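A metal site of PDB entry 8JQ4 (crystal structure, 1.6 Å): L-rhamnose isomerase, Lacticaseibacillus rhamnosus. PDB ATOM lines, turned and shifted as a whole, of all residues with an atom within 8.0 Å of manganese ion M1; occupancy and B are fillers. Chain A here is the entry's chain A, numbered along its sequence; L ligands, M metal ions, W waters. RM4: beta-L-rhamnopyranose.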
ATOM      1  N   TRP A 187      13.607 -24.704  20.383  1.00  0.00           N
ATOM      2  CA  TRP A 187      13.103 -23.302  20.397  1.00  0.00           C
ATOM      3  C   TRP A 187      14.291 -22.344  20.441  1.00  0.00           C
ATOM      4  O   TRP A 187      15.144 -22.496  21.328  1.00  0.00           O
ATOM      5  CB  TRP A 187      12.159 -23.058  21.569  1.00  0.00           C
ATOM      6  CG  TRP A 187      11.707 -21.632  21.575  1.00  0.00           C
ATOM      7  CD1 TRP A 187      10.858 -21.046  20.677  1.00  0.00           C
ATOM      8  CD2 TRP A 187      12.240 -20.571  22.387  1.00  0.00           C
ATOM      9  NE1 TRP A 187      10.797 -19.701  20.904  1.00  0.00           N
ATOM     10  CE2 TRP A 187      11.612 -19.379  21.951  1.00  0.00           C
ATOM     11  CE3 TRP A 187      13.166 -20.506  23.440  1.00  0.00           C
ATOM     12  CZ2 TRP A 187      11.875 -18.147  22.561  1.00  0.00           C
ATOM     13  CZ3 TRP A 187      13.409 -19.287  24.032  1.00  0.00           C
ATOM     14  CH2 TRP A 187      12.775 -18.127  23.601  1.00  0.00           C
ATOM     15  N   GLU A 228       9.839 -25.484  17.207  1.00  0.00           N
ATOM     16  CA  GLU A 228       8.852 -24.601  17.890  1.00  0.00           C
ATOM     17  C   GLU A 228       9.033 -23.157  17.409  1.00  0.00           C
ATOM     18  O   GLU A 228      10.091 -22.558  17.703  1.00  0.00           O
ATOM     19  CB  GLU A 228       8.988 -24.683  19.397  1.00  0.00           C
ATOM     20  CG  GLU A 228       7.976 -23.799  20.118  1.00  0.00           C
ATOM     21  CD  GLU A 228       8.042 -23.906  21.621  1.00  0.00           C
ATOM     22  OE1 GLU A 228       8.927 -24.618  22.137  1.00  0.00           O
ATOM     23  OE2 GLU A 228       7.204 -23.262  22.283  1.00  0.00           O
ATOM     24  N   LYS A 230       7.370 -19.042  17.181  1.00  0.00           N
ATOM     25  CA  LYS A 230       6.816 -18.028  18.106  1.00  0.00           C
ATOM     26  C   LYS A 230       6.465 -16.802  17.274  1.00  0.00           C
ATOM     27  O   LYS A 230       7.126 -16.597  16.246  1.00  0.00           O
ATOM     28  CB  LYS A 230       7.861 -17.718  19.182  1.00  0.00           C
ATOM     29  CG  LYS A 230       7.337 -17.084  20.458  1.00  0.00           C
ATOM     30  CD  LYS A 230       8.392 -17.010  21.526  1.00  0.00           C
ATOM     31  CE  LYS A 230       7.898 -16.454  22.838  1.00  0.00           C
ATOM     32  NZ  LYS A 230       8.977 -16.420  23.852  1.00  0.00           N
ATOM     33  N   PHE A 232       6.147 -13.551  18.710  1.00  0.00           N
ATOM     34  CA  PHE A 232       6.913 -12.434  19.334  1.00  0.00           C
ATOM     35  C   PHE A 232       7.252 -12.776  20.789  1.00  0.00           C
ATOM     36  O   PHE A 232       6.502 -13.517  21.441  1.00  0.00           O
ATOM     37  CB  PHE A 232       6.125 -11.129  19.259  1.00  0.00           C
ATOM     38  CG  PHE A 232       5.045 -10.974  20.298  1.00  0.00           C
ATOM     39  CD1 PHE A 232       5.265 -10.223  21.437  1.00  0.00           C
ATOM     40  CD2 PHE A 232       3.803 -11.586  20.152  1.00  0.00           C
ATOM     41  CE1 PHE A 232       4.282 -10.066  22.402  1.00  0.00           C
ATOM     42  CE2 PHE A 232       2.814 -11.426  21.111  1.00  0.00           C
ATOM     43  CZ  PHE A 232       3.056 -10.668  22.232  1.00  0.00           C
ATOM     44  N   ASP A 261       2.803 -24.201  20.477  1.00  0.00           N
ATOM     45  CA  ASP A 261       2.610 -23.666  21.848  1.00  0.00           C
ATOM     46  C   ASP A 261       1.412 -22.716  21.821  1.00  0.00           C
ATOM     47  O   ASP A 261       1.440 -21.764  21.014  1.00  0.00           O
ATOM     48  CB  ASP A 261       3.889 -23.019  22.380  1.00  0.00           C
ATOM     49  CG  ASP A 261       3.754 -22.503  23.804  1.00  0.00           C
ATOM     50  OD1 ASP A 261       4.597 -22.882  24.648  1.00  0.00           O
ATOM     51  OD2 ASP A 261       2.798 -21.740  24.055  1.00  0.00           O
ATOM     52  N   ALA A 262       0.394 -22.989  22.642  1.00  0.00           N
ATOM     53  CA  ALA A 262      -0.933 -22.322  22.612  1.00  0.00           C
ATOM     54  C   ALA A 262      -0.785 -20.848  22.996  1.00  0.00           C
ATOM     55  O   ALA A 262      -1.720 -20.076  22.728  1.00  0.00           O
ATOM     56  CB  ALA A 262      -1.884 -23.039  23.531  1.00  0.00           C
ATOM     57  N   GLY A 263       0.370 -20.441  23.512  1.00  0.00           N
ATOM     58  CA  GLY A 263       0.621 -19.055  23.961  1.00  0.00           C
ATOM     59  C   GLY A 263       1.277 -18.187  22.895  1.00  0.00           C
ATOM     60  O   GLY A 263       1.482 -17.005  23.159  1.00  0.00           O
ATOM     61  N   HIS A 264       1.664 -18.759  21.746  1.00  0.00           N
ATOM     62  CA  HIS A 264       2.689 -18.155  20.848  1.00  0.00           C
ATOM     63  C   HIS A 264       2.072 -17.643  19.543  1.00  0.00           C
ATOM     64  O   HIS A 264       2.848 -17.366  18.602  1.00  0.00           O
ATOM     65  CB  HIS A 264       3.832 -19.152  20.614  1.00  0.00           C
ATOM     66  CG  HIS A 264       4.633 -19.413  21.842  1.00  0.00           C
ATOM     67  ND1 HIS A 264       5.786 -20.174  21.829  1.00  0.00           N
ATOM     68  CD2 HIS A 264       4.475 -18.986  23.115  1.00  0.00           C
ATOM     69  CE1 HIS A 264       6.273 -20.229  23.054  1.00  0.00           C
ATOM     70  NE2 HIS A 264       5.497 -19.503  23.858  1.00  0.00           N
ATOM     71  N   HIS A 288       2.149 -27.968  22.973  1.00  0.00           N
ATOM     72  CA  HIS A 288       2.519 -27.324  24.254  1.00  0.00           C
ATOM     73  C   HIS A 288       1.341 -26.485  24.761  1.00  0.00           C
ATOM     74  O   HIS A 288       1.134 -25.400  24.204  1.00  0.00           O
ATOM     75  CB  HIS A 288       3.737 -26.406  24.078  1.00  0.00           C
ATOM     76  CG  HIS A 288       5.018 -27.159  24.009  1.00  0.00           C
ATOM     77  ND1 HIS A 288       6.238 -26.529  24.169  1.00  0.00           N
ATOM     78  CD2 HIS A 288       5.276 -28.465  23.822  1.00  0.00           C
ATOM     79  CE1 HIS A 288       7.196 -27.432  24.049  1.00  0.00           C
ATOM     80  NE2 HIS A 288       6.626 -28.623  23.844  1.00  0.00           N
ATOM     81  N   VAL A 289       0.606 -26.995  25.755  1.00  0.00           N
ATOM     82  CA  VAL A 289      -0.520 -26.216  26.343  1.00  0.00           C
ATOM     83  C   VAL A 289       0.073 -25.206  27.320  1.00  0.00           C
ATOM     84  O   VAL A 289       0.959 -25.561  28.121  1.00  0.00           O
ATOM     85  CB  VAL A 289      -1.606 -27.091  26.979  1.00  0.00           C
ATOM     86  CG1 VAL A 289      -2.348 -27.885  25.912  1.00  0.00           C
ATOM     87  CG2 VAL A 289      -1.072 -27.999  28.069  1.00  0.00           C
ATOM     88  N   SER A 290      -0.369 -23.955  27.174  1.00  0.00           N
ATOM     89  CA  SER A 290       0.107 -22.756  27.903  1.00  0.00           C
ATOM     90  C   SER A 290      -1.004 -21.723  27.792  1.00  0.00           C
ATOM     91  O   SER A 290      -1.694 -21.719  26.757  1.00  0.00           O
ATOM     92  CB  SER A 290       1.403 -22.253  27.312  1.00  0.00           C
ATOM     93  OG  SER A 290       1.938 -21.200  28.089  1.00  0.00           O
ATOM     94  N   ARG A 291      -1.216 -20.913  28.823  1.00  0.00           N
ATOM     95  CA  ARG A 291      -2.247 -19.844  28.815  1.00  0.00           C
ATOM     96  C   ARG A 291      -1.575 -18.499  28.583  1.00  0.00           C
ATOM     97  O   ARG A 291      -0.870 -17.992  29.461  1.00  0.00           O
ATOM     98  CB  ARG A 291      -3.063 -19.835  30.104  1.00  0.00           C
ATOM     99  CG  ARG A 291      -4.029 -18.654  30.204  1.00  0.00           C
ATOM    100  CD  ARG A 291      -5.101 -18.882  31.240  1.00  0.00           C
ATOM    101  NE  ARG A 291      -4.508 -19.271  32.511  1.00  0.00           N
ATOM    102  CZ  ARG A 291      -4.604 -18.579  33.637  1.00  0.00           C
ATOM    103  NH1 ARG A 291      -4.000 -19.023  34.728  1.00  0.00           N
ATOM    104  NH2 ARG A 291      -5.315 -17.469  33.686  1.00  0.00           N
ATOM    105  N   PRO A 292      -1.794 -17.877  27.412  1.00  0.00           N
ATOM    106  CA  PRO A 292      -1.420 -16.484  27.203  1.00  0.00           C
ATOM    107  C   PRO A 292      -2.503 -15.564  27.777  1.00  0.00           C
ATOM    108  O   PRO A 292      -3.659 -15.784  27.510  1.00  0.00           O
ATOM    109  CB  PRO A 292      -1.348 -16.369  25.679  1.00  0.00           C
ATOM    110  CG  PRO A 292      -2.432 -17.323  25.209  1.00  0.00           C
ATOM    111  CD  PRO A 292      -2.421 -18.465  26.221  1.00  0.00           C
ATOM    112  N   TRP A 295      -0.355 -11.505  26.150  1.00  0.00           N
ATOM    113  CA  TRP A 295       0.944 -11.797  25.492  1.00  0.00           C
ATOM    114  C   TRP A 295       1.379 -13.214  25.853  1.00  0.00           C
ATOM    115  O   TRP A 295       0.588 -13.926  26.498  1.00  0.00           O
ATOM    116  CB  TRP A 295       2.003 -10.755  25.868  1.00  0.00           C
ATOM    117  CG  TRP A 295       2.490 -10.861  27.287  1.00  0.00           C
ATOM    118  CD1 TRP A 295       1.763 -10.632  28.425  1.00  0.00           C
ATOM    119  CD2 TRP A 295       3.811 -11.217  27.730  1.00  0.00           C
ATOM    120  NE1 TRP A 295       2.543 -10.825  29.532  1.00  0.00           N
ATOM    121  CE2 TRP A 295       3.796 -11.194  29.139  1.00  0.00           C
ATOM    122  CE3 TRP A 295       4.999 -11.588  27.079  1.00  0.00           C
ATOM    123  CZ2 TRP A 295       4.923 -11.496  29.902  1.00  0.00           C
ATOM    124  CZ3 TRP A 295       6.108 -11.892  27.830  1.00  0.00           C
ATOM    125  CH2 TRP A 295       6.068 -11.854  29.225  1.00  0.00           C
ATOM    126  N   ASP A 296       2.563 -13.628  25.415  1.00  0.00           N
ATOM    127  CA  ASP A 296       3.154 -14.929  25.803  1.00  0.00           C
ATOM    128  C   ASP A 296       3.575 -14.886  27.281  1.00  0.00           C
ATOM    129  O   ASP A 296       4.791 -14.859  27.558  1.00  0.00           O
ATOM    130  CB  ASP A 296       4.349 -15.288  24.920  1.00  0.00           C
ATOM    131  CG  ASP A 296       4.950 -16.623  25.297  1.00  0.00           C
ATOM    132  OD1 ASP A 296       4.176 -17.478  25.786  1.00  0.00           O
ATOM    133  OD2 ASP A 296       6.173 -16.784  25.146  1.00  0.00           O
ATOM    134  N   SER A 297       2.586 -14.939  28.179  1.00  0.00           N
ATOM    135  CA  SER A 297       2.726 -14.670  29.636  1.00  0.00           C
ATOM    136  C   SER A 297       3.028 -15.962  30.395  1.00  0.00           C
ATOM    137  O   SER A 297       3.405 -15.880  31.586  1.00  0.00           O
ATOM    138  CB  SER A 297       1.494 -14.000  30.169  1.00  0.00           C
ATOM    139  OG  SER A 297       0.341 -14.800  29.908  1.00  0.00           O
ATOM    140  N   ASP A 298       2.773 -17.113  29.774  1.00  0.00           N
ATOM    141  CA  ASP A 298       3.084 -18.463  30.339  1.00  0.00           C
ATOM    142  C   ASP A 298       2.337 -18.634  31.665  1.00  0.00           C
ATOM    143  O   ASP A 298       2.920 -19.176  32.626  1.00  0.00           O
ATOM    144  CB  ASP A 298       4.595 -18.630  30.468  1.00  0.00           C
ATOM    145  CG  ASP A 298       5.274 -18.729  29.103  1.00  0.00           C
ATOM    146  OD1 ASP A 298       4.605 -19.164  28.156  1.00  0.00           O
ATOM    147  OD2 ASP A 298       6.435 -18.308  29.001  1.00  0.00           O
ATOM    148  N   HIS A 299       1.056 -18.239  31.706  1.00  0.00           N
ATOM    149  CA  HIS A 299       0.135 -18.549  32.823  1.00  0.00           C
ATOM    150  C   HIS A 299      -0.123 -20.057  32.884  1.00  0.00           C
ATOM    151  O   HIS A 299      -0.072 -20.728  31.823  1.00  0.00           O
ATOM    152  CB  HIS A 299      -1.176 -17.764  32.691  1.00  0.00           C
ATOM    153  CG  HIS A 299      -1.086 -16.358  33.154  1.00  0.00           C
ATOM    154  ND1 HIS A 299      -0.324 -15.411  32.504  1.00  0.00           N
ATOM    155  CD2 HIS A 299      -1.685 -15.716  34.186  1.00  0.00           C
ATOM    156  CE1 HIS A 299      -0.453 -14.244  33.111  1.00  0.00           C
ATOM    157  NE2 HIS A 299      -1.285 -14.408  34.158  1.00  0.00           N
ATOM    158  N   ASP A 328       3.682 -26.086  29.241  1.00  0.00           N
ATOM    159  CA  ASP A 328       4.671 -24.981  29.294  1.00  0.00           C
ATOM    160  C   ASP A 328       4.010 -23.786  29.971  1.00  0.00           C
ATOM    161  O   ASP A 328       3.065 -23.191  29.397  1.00  0.00           O
ATOM    162  CB  ASP A 328       5.226 -24.652  27.918  1.00  0.00           C
ATOM    163  CG  ASP A 328       6.577 -23.963  27.972  1.00  0.00           C
ATOM    164  OD1 ASP A 328       7.147 -23.725  26.898  1.00  0.00           O
ATOM    165  OD2 ASP A 328       7.046 -23.636  29.095  1.00  0.00           O
ATOM    166  N   PHE A 329       4.459 -23.475  31.191  1.00  0.00           N
ATOM    167  CA  PHE A 329       4.045 -22.269  31.950  1.00  0.00           C
ATOM    168  C   PHE A 329       5.052 -22.023  33.073  1.00  0.00           C
ATOM    169  O   PHE A 329       5.793 -22.952  33.415  1.00  0.00           O
ATOM    170  CB  PHE A 329       2.605 -22.406  32.460  1.00  0.00           C
ATOM    171  CG  PHE A 329       2.254 -23.714  33.120  1.00  0.00           C
ATOM    172  CD1 PHE A 329       2.627 -23.973  34.425  1.00  0.00           C
ATOM    173  CD2 PHE A 329       1.450 -24.644  32.476  1.00  0.00           C
ATOM    174  CE1 PHE A 329       2.258 -25.149  35.050  1.00  0.00           C
ATOM    175  CE2 PHE A 329       1.081 -25.821  33.101  1.00  0.00           C
ATOM    176  CZ  PHE A 329       1.476 -26.073  34.389  1.00  0.00           C
ATOM    177  N   PHE A 330       5.203 -20.760  33.483  1.00  0.00           N
ATOM    178  CA  PHE A 330       5.878 -20.286  34.718  1.00  0.00           C
ATOM    179  C   PHE A 330       4.851 -19.579  35.570  1.00  0.00           C
ATOM    180  O   PHE A 330       4.249 -18.602  35.094  1.00  0.00           O
ATOM    181  CB  PHE A 330       6.946 -19.213  34.453  1.00  0.00           C
ATOM    182  CG  PHE A 330       8.096 -19.670  33.608  1.00  0.00           C
ATOM    183  CD1 PHE A 330       9.204 -20.270  34.188  1.00  0.00           C
ATOM    184  CD2 PHE A 330       8.067 -19.490  32.236  1.00  0.00           C
ATOM    185  CE1 PHE A 330      10.267 -20.690  33.398  1.00  0.00           C
ATOM    186  CE2 PHE A 330       9.130 -19.910  31.445  1.00  0.00           C
ATOM    187  CZ  PHE A 330      10.234 -20.505  32.032  1.00  0.00           C
HETATM  188  C1  RM4 L   1      10.039 -20.348  25.225  1.00  0.00           C
HETATM  189  C2  RM4 L   1       9.390 -21.570  24.630  1.00  0.00           C
HETATM  190  C3  RM4 L   1      10.244 -22.821  24.843  1.00  0.00           C
HETATM  191  C4  RM4 L   1      10.744 -22.958  26.278  1.00  0.00           C
HETATM  192  C5  RM4 L   1      11.279 -21.640  26.808  1.00  0.00           C
HETATM  193  C6  RM4 L   1      11.587 -21.690  28.287  1.00  0.00           C
HETATM  194  O1  RM4 L   1       9.196 -19.249  25.044  1.00  0.00           O
HETATM  195  O2  RM4 L   1       8.068 -21.714  25.157  1.00  0.00           O
HETATM  196  O3  RM4 L   1       9.487 -23.978  24.494  1.00  0.00           O
HETATM  197  O4  RM4 L   1      11.797 -23.925  26.314  1.00  0.00           O
HETATM  198  O5  RM4 L   1      10.293 -20.603  26.613  1.00  0.00           O
HETATM  199 MN    MN M   1       5.032 -19.181  26.140  1.00  0.00          MN
HETATM  200 MN    MN M   2       6.729 -23.860  24.508  1.00  0.00          MN
HETATM  201  O   HOH W   1       3.075 -20.050  25.968  1.00  0.00           O
HETATM  202  O   HOH W   2       5.551 -21.128  26.414  1.00  0.00           O
HETATM  203  O   HOH W   3       7.069 -18.636  26.488  1.00  0.00           O
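NZ of Lys 230 is in hydrogen-bond range of O1 of the ligand (3.1 Å).
OD2 of Asp 296 is in salt-bridge range of NZ of Lys 230.
The side-chain carboxylate of Glu 228 lies close to a ring nitrogen (ND1) of His 264, 3.4 Å away.
O of Asp 298 sits at hydrogen-bond distance from N of Phe 330, at 2.9 Å.
OD2 of Asp 261 lies within hydrogen-bond range of N of Gly 263.
The side-chain carboxylate of Asp 298 lies close to the side-chain hydroxyl of Ser 290 (3.4 Å).
Merely in contact with manganese ion M1: Asp 261.
Within 4 Å of manganese ion M1: Asp 261, His 264, Asp 296 and Asp 298.
The nearest printed residue that does not touch manganese ion M1 is Ser 290 (4.2 Å).
Manganese ion M1 is bound by the side-chain carboxylate (OD1) of Asp 296 (1.9 Å), water W2 (2.0 Å), the side-chain carboxylate (OD1) of Asp 298 (2.1 Å), water W3 (2.1 Å), water W1 (2.1 Å) and a ring nitrogen (NE2) of His 264 (2.4 Å).
Manganese ion M1 has six donor atoms within binding distance.
Slightly farther from manganese ion M1 lies the side-chain carboxylate (OD2) of Asp 296 (2.8 Å).
Water W1 bridges the side-chain carboxylate of Asp 261 and the side-chain hydroxyl of Ser 290.
Water W3 lies within hydrogen-bond range of the side-chain carboxylate (OD2) of Asp 296, the side-chain carboxylate (OD2) of Asp 298 and an oxygen (O1) of the ligand.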
